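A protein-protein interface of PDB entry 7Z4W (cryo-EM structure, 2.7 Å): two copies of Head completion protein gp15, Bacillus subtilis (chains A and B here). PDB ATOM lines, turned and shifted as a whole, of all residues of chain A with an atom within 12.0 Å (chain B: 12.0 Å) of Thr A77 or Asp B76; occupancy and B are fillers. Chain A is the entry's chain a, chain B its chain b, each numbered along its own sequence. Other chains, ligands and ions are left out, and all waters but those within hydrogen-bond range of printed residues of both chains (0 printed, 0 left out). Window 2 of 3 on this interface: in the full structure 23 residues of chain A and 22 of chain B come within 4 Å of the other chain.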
ATOM      1  N   ARG A  73     -24.256  21.842 -16.833  1.00  0.00           N
ATOM      2  CA  ARG A  73     -24.133  23.292 -16.910  1.00  0.00           C
ATOM      3  C   ARG A  73     -23.681  23.847 -15.567  1.00  0.00           C
ATOM      4  O   ARG A  73     -24.091  23.350 -14.519  1.00  0.00           O
ATOM      5  CB  ARG A  73     -25.463  23.924 -17.333  1.00  0.00           C
ATOM      6  CG  ARG A  73     -25.339  25.312 -17.885  1.00  0.00           C
ATOM      7  CD  ARG A  73     -26.616  25.745 -18.570  1.00  0.00           C
ATOM      8  NE  ARG A  73     -27.703  25.996 -17.633  1.00  0.00           N
ATOM      9  CZ  ARG A  73     -27.906  27.161 -17.029  1.00  0.00           C
ATOM     10  NH1 ARG A  73     -28.921  27.310 -16.192  1.00  0.00           N
ATOM     11  NH2 ARG A  73     -27.089  28.176 -17.261  1.00  0.00           N
ATOM     12  N   SER A  74     -22.831  24.873 -15.600  1.00  0.00           N
ATOM     13  CA  SER A  74     -22.339  25.519 -14.388  1.00  0.00           C
ATOM     14  C   SER A  74     -22.351  27.032 -14.555  1.00  0.00           C
ATOM     15  O   SER A  74     -22.014  27.549 -15.623  1.00  0.00           O
ATOM     16  CB  SER A  74     -20.932  25.036 -14.036  1.00  0.00           C
ATOM     17  OG  SER A  74     -20.459  25.657 -12.860  1.00  0.00           O
ATOM     18  N   MET A  75     -22.748  27.731 -13.495  1.00  0.00           N
ATOM     19  CA  MET A  75     -22.897  29.186 -13.474  1.00  0.00           C
ATOM     20  C   MET A  75     -22.660  29.595 -12.029  1.00  0.00           C
ATOM     21  O   MET A  75     -23.435  29.185 -11.173  1.00  0.00           O
ATOM     22  CB  MET A  75     -24.291  29.593 -13.947  1.00  0.00           C
ATOM     23  CG  MET A  75     -24.611  31.063 -13.842  1.00  0.00           C
ATOM     24  SD  MET A  75     -26.346  31.410 -14.198  1.00  0.00           S
ATOM     25  CE  MET A  75     -27.158  30.021 -13.419  1.00  0.00           C
ATOM     26  N   ASP A  76     -21.463  30.150 -11.869  1.00  0.00           N
ATOM     27  CA  ASP A  76     -20.807  30.594 -10.646  1.00  0.00           C
ATOM     28  C   ASP A  76     -20.950  29.594  -9.525  1.00  0.00           C
ATOM     29  O   ASP A  76     -20.159  28.690  -9.403  1.00  0.00           O
ATOM     30  CB  ASP A  76     -21.193  32.020 -10.217  1.00  0.00           C
ATOM     31  CG  ASP A  76     -20.165  32.665  -9.277  1.00  0.00           C
ATOM     32  OD1 ASP A  76     -19.260  32.002  -8.761  1.00  0.00           O
ATOM     33  OD2 ASP A  76     -20.255  33.875  -9.037  1.00  0.00           O
ATOM     34  N   THR A  77     -21.999  29.730  -8.742  1.00  0.00           N
ATOM     35  CA  THR A  77     -22.200  28.857  -7.584  1.00  0.00           C
ATOM     36  C   THR A  77     -23.229  27.752  -7.811  1.00  0.00           C
ATOM     37  O   THR A  77     -23.259  26.790  -7.038  1.00  0.00           O
ATOM     38  CB  THR A  77     -22.593  29.678  -6.348  1.00  0.00           C
ATOM     39  OG1 THR A  77     -23.725  30.502  -6.646  1.00  0.00           O
ATOM     40  CG2 THR A  77     -21.436  30.539  -5.884  1.00  0.00           C
ATOM     41  N   VAL A  78     -24.064  27.878  -8.816  1.00  0.00           N
ATOM     42  CA  VAL A  78     -25.104  26.927  -9.189  1.00  0.00           C
ATOM     43  C   VAL A  78     -24.579  25.975 -10.264  1.00  0.00           C
ATOM     44  O   VAL A  78     -23.775  26.357 -11.118  1.00  0.00           O
ATOM     45  CB  VAL A  78     -26.351  27.716  -9.656  1.00  0.00           C
ATOM     46  CG1 VAL A  78     -27.545  26.812  -9.935  1.00  0.00           C
ATOM     47  CG2 VAL A  78     -26.711  28.771  -8.630  1.00  0.00           C
ATOM     48  N   SER A  79     -25.020  24.718 -10.225  1.00  0.00           N
ATOM     49  CA  SER A  79     -24.704  23.773 -11.289  1.00  0.00           C
ATOM     50  C   SER A  79     -25.841  22.771 -11.442  1.00  0.00           C
ATOM     51  O   SER A  79     -26.606  22.523 -10.511  1.00  0.00           O
ATOM     52  CB  SER A  79     -23.380  23.047 -11.028  1.00  0.00           C
ATOM     53  OG  SER A  79     -23.333  22.512  -9.721  1.00  0.00           O
ATOM     54  N   TYR A  80     -25.935  22.194 -12.642  1.00  0.00           N
ATOM     55  CA  TYR A  80     -26.966  21.225 -12.991  1.00  0.00           C
ATOM     56  C   TYR A  80     -26.375  20.080 -13.799  1.00  0.00           C
ATOM     57  O   TYR A  80     -25.516  20.295 -14.659  1.00  0.00           O
ATOM     58  CB  TYR A  80     -28.095  21.854 -13.815  1.00  0.00           C
ATOM     59  CG  TYR A  80     -28.760  23.051 -13.195  1.00  0.00           C
ATOM     60  CD1 TYR A  80     -29.671  22.904 -12.158  1.00  0.00           C
ATOM     61  CD2 TYR A  80     -28.499  24.331 -13.663  1.00  0.00           C
ATOM     62  CE1 TYR A  80     -30.285  23.999 -11.589  1.00  0.00           C
ATOM     63  CE2 TYR A  80     -29.110  25.434 -13.103  1.00  0.00           C
ATOM     64  CZ  TYR A  80     -30.003  25.260 -12.069  1.00  0.00           C
ATOM     65  OH  TYR A  80     -30.616  26.354 -11.508  1.00  0.00           O
ATOM     66  N   ASN A  81     -26.860  18.870 -13.527  1.00  0.00           N
ATOM     67  CA  ASN A  81     -26.583  17.681 -14.322  1.00  0.00           C
ATOM     68  C   ASN A  81     -27.904  17.131 -14.839  1.00  0.00           C
ATOM     69  O   ASN A  81     -28.837  16.925 -14.060  1.00  0.00           O
ATOM     70  CB  ASN A  81     -25.860  16.609 -13.505  1.00  0.00           C
ATOM     71  CG  ASN A  81     -24.429  16.977 -13.197  1.00  0.00           C
ATOM     72  OD1 ASN A  81     -23.566  16.938 -14.069  1.00  0.00           O
ATOM     73  ND2 ASN A  81     -24.166  17.332 -11.947  1.00  0.00           N
ATOM     74  N   GLY B  72     -28.678  15.793 -10.865  1.00  0.00           N
ATOM     75  CA  GLY B  72     -27.921  16.423  -9.799  1.00  0.00           C
ATOM     76  C   GLY B  72     -28.110  17.921  -9.804  1.00  0.00           C
ATOM     77  O   GLY B  72     -28.406  18.525 -10.837  1.00  0.00           O
ATOM     78  N   ARG B  73     -27.923  18.520  -8.630  1.00  0.00           N
ATOM     79  CA  ARG B  73     -28.154  19.949  -8.452  1.00  0.00           C
ATOM     80  C   ARG B  73     -27.266  20.460  -7.324  1.00  0.00           C
ATOM     81  O   ARG B  73     -26.924  19.710  -6.412  1.00  0.00           O
ATOM     82  CB  ARG B  73     -29.636  20.222  -8.153  1.00  0.00           C
ATOM     83  CG  ARG B  73     -30.070  21.651  -8.329  1.00  0.00           C
ATOM     84  CD  ARG B  73     -31.585  21.817  -8.271  1.00  0.00           C
ATOM     85  NE  ARG B  73     -32.191  21.436  -6.996  1.00  0.00           N
ATOM     86  CZ  ARG B  73     -32.136  22.147  -5.871  1.00  0.00           C
ATOM     87  NH1 ARG B  73     -32.742  21.700  -4.784  1.00  0.00           N
ATOM     88  NH2 ARG B  73     -31.477  23.295  -5.816  1.00  0.00           N
ATOM     89  N   SER B  74     -26.882  21.736  -7.393  1.00  0.00           N
ATOM     90  CA  SER B  74     -26.027  22.320  -6.363  1.00  0.00           C
ATOM     91  C   SER B  74     -26.236  23.825  -6.274  1.00  0.00           C
ATOM     92  O   SER B  74     -26.260  24.505  -7.300  1.00  0.00           O
ATOM     93  CB  SER B  74     -24.554  22.016  -6.649  1.00  0.00           C
ATOM     94  OG  SER B  74     -23.722  22.588  -5.663  1.00  0.00           O
ATOM     95  N   MET B  75     -26.402  24.342  -5.050  1.00  0.00           N
ATOM     96  CA  MET B  75     -26.447  25.788  -4.797  1.00  0.00           C
ATOM     97  C   MET B  75     -25.652  26.114  -3.529  1.00  0.00           C
ATOM     98  O   MET B  75     -26.166  26.016  -2.409  1.00  0.00           O
ATOM     99  CB  MET B  75     -27.881  26.285  -4.706  1.00  0.00           C
ATOM    100  CG  MET B  75     -27.991  27.797  -4.693  1.00  0.00           C
ATOM    101  SD  MET B  75     -29.493  28.395  -5.476  1.00  0.00           S
ATOM    102  CE  MET B  75     -30.662  28.100  -4.171  1.00  0.00           C
ATOM    103  N   ASP B  76     -24.357  26.372  -3.713  1.00  0.00           N
ATOM    104  CA  ASP B  76     -23.459  27.156  -2.861  1.00  0.00           C
ATOM    105  C   ASP B  76     -23.115  26.578  -1.486  1.00  0.00           C
ATOM    106  O   ASP B  76     -21.998  26.779  -1.001  1.00  0.00           O
ATOM    107  CB  ASP B  76     -24.072  28.551  -2.670  1.00  0.00           C
ATOM    108  CG  ASP B  76     -23.247  29.440  -1.761  1.00  0.00           C
ATOM    109  OD1 ASP B  76     -22.120  29.812  -2.143  1.00  0.00           O
ATOM    110  OD2 ASP B  76     -23.727  29.761  -0.656  1.00  0.00           O
ATOM    111  N   THR B  77     -23.987  25.757  -0.913  1.00  0.00           N
ATOM    112  CA  THR B  77     -23.716  25.022   0.318  1.00  0.00           C
ATOM    113  C   THR B  77     -24.477  23.715   0.222  1.00  0.00           C
ATOM    114  O   THR B  77     -24.116  22.724   0.859  1.00  0.00           O
ATOM    115  CB  THR B  77     -24.133  25.780   1.595  1.00  0.00           C
ATOM    116  OG1 THR B  77     -25.396  26.429   1.411  1.00  0.00           O
ATOM    117  CG2 THR B  77     -23.081  26.783   2.059  1.00  0.00           C
ATOM    118  N   VAL B  78     -25.538  23.718  -0.574  1.00  0.00           N
ATOM    119  CA  VAL B  78     -26.430  22.575  -0.686  1.00  0.00           C
ATOM    120  C   VAL B  78     -26.122  21.842  -1.985  1.00  0.00           C
ATOM    121  O   VAL B  78     -25.748  22.457  -2.985  1.00  0.00           O
ATOM    122  CB  VAL B  78     -27.899  23.045  -0.621  1.00  0.00           C
ATOM    123  CG1 VAL B  78     -28.815  21.899  -0.324  1.00  0.00           C
ATOM    124  CG2 VAL B  78     -28.062  24.129   0.423  1.00  0.00           C
ATOM    125  N   SER B  79     -26.260  20.516  -1.974  1.00  0.00           N
ATOM    126  CA  SER B  79     -26.141  19.731  -3.194  1.00  0.00           C
ATOM    127  C   SER B  79     -26.976  18.464  -3.064  1.00  0.00           C
ATOM    128  O   SER B  79     -27.193  17.957  -1.963  1.00  0.00           O
ATOM    129  CB  SER B  79     -24.681  19.385  -3.510  1.00  0.00           C
ATOM    130  OG  SER B  79     -24.290  18.172  -2.903  1.00  0.00           O
ATOM    131  N   TYR B  80     -27.438  17.960  -4.209  1.00  0.00           N
ATOM    132  CA  TYR B  80     -28.298  16.788  -4.282  1.00  0.00           C
ATOM    133  C   TYR B  80     -27.909  15.916  -5.463  1.00  0.00           C
ATOM    134  O   TYR B  80     -27.613  16.421  -6.550  1.00  0.00           O
ATOM    135  CB  TYR B  80     -29.774  17.160  -4.437  1.00  0.00           C
ATOM    136  CG  TYR B  80     -30.326  17.999  -3.327  1.00  0.00           C
ATOM    137  CD1 TYR B  80     -30.671  17.430  -2.111  1.00  0.00           C
ATOM    138  CD2 TYR B  80     -30.504  19.361  -3.493  1.00  0.00           C
ATOM    139  CE1 TYR B  80     -31.174  18.197  -1.090  1.00  0.00           C
ATOM    140  CE2 TYR B  80     -31.008  20.133  -2.484  1.00  0.00           C
ATOM    141  CZ  TYR B  80     -31.340  19.550  -1.282  1.00  0.00           C
ATOM    142  OH  TYR B  80     -31.845  20.330  -0.271  1.00  0.00           O
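OG of Ser B74 is in hydrogen-bond range of O of Val B78 (3.4 Å). The backbone carbonyl oxygen (O) of Arg B73 is in hydrogen-bond range of the backbone NH (N) of Tyr B80, 2.9 Å away. The backbone carbonyl oxygen of Arg A73 lies within hydrogen-bond range of the backbone NH of Tyr A80, at 2.9 Å.
N of Asn A81 is in hydrogen-bond range of O of Gly B72. The backbone NH (N) of Ser A79 sits at hydrogen-bond distance from the backbone carbonyl oxygen (O) of Ser B74 (3.2 Å).
Thr A77 touches Asp B76, but with the chains exchanged Asp A76 does not touch Thr B77 (9.8 Å). Val A78 touches Ser B74, but with the chains exchanged Ser A74 does not touch Val B78 (11.7 Å). Ser A79 touches Arg B73, but with the chains exchanged Arg A73 does not touch Ser B79 (11.7 Å). Ser A79 touches Ser B74, but with the chains exchanged Ser A74 does not touch Ser B79 (12.0 Å). 8 positions are printed for both chains. Of the 7 pairs that touch across the chains among the printed residues, none has its exchanged pair printed and touching as well.
Of the 9 printed residues of chain A, 5 touch a printed residue of chain B. Printed residues of chain A that touch a printed residue of chain B: Thr A77, Val A78, Ser A79, Tyr A80 and Asn A81. Along chain A the printed residues that touch a printed residue of chain B span positions 77 to 81. Among the printed residues, 7 pairs touch across the chains. Among the printed residues, no Asp or Glu carboxylate lies within 4 Å of a Lys or Arg side-chain nitrogen of the other chain.
Thr A77 touches just these residues of chain B: Ser B74 (3.8 Å) and Asp B76 (3.5 Å). Of the printed residues of chain A, Asp B76 touches Thr A77. Met A75 touches none of the printed residues of chain B. No residue of chain B comes within 4 Å of Asp A76. Val A78 touches just one residue of chain B: Ser B74. Of chain B, only Arg B73 (3.6 Å) and Ser B74 (3.2 Å) come within 4 Å of Ser A79. Printed residues of chain A within 4 Å of Ser B74: Thr A77 (3.8 Å), Val A78 (3.3 Å) and Ser A79 (3.2 Å). No residue of chain A comes within 4 Å of Met B75. Val B78 touches none of the printed residues of chain A. Printed residues of chain B within 4 Å of Tyr A80: Gly B72 (3.7 Å). Of the printed residues of chain B, Asn A81 touches Gly B72 (3.1 Å). Of the printed residues of chain A, Gly B72 touches Tyr A80 and Asn A81. Of the printed residues of chain A, Arg B73 touches Ser A79. Ser A74 touches none of the printed residues of chain B. Ser B79 touches none of the printed residues of chain A. The nearest residue of chain B that does not touch Thr A77 is Met B75 (4.02 Å). The nearest printed residue of chain B that does not touch Asn A81 is Arg B73 (5.0 Å).
Among the printed residues, pairs that only touch across the chains: Val A78 with Ser B74 (3.3 Å), Thr A77 with Asp B76 (3.5 Å), Ser A79 with Arg B73 (3.6 Å), Tyr A80 with Gly B72 (3.7 Å) and Thr A77 with Ser B74 (3.8 Å).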
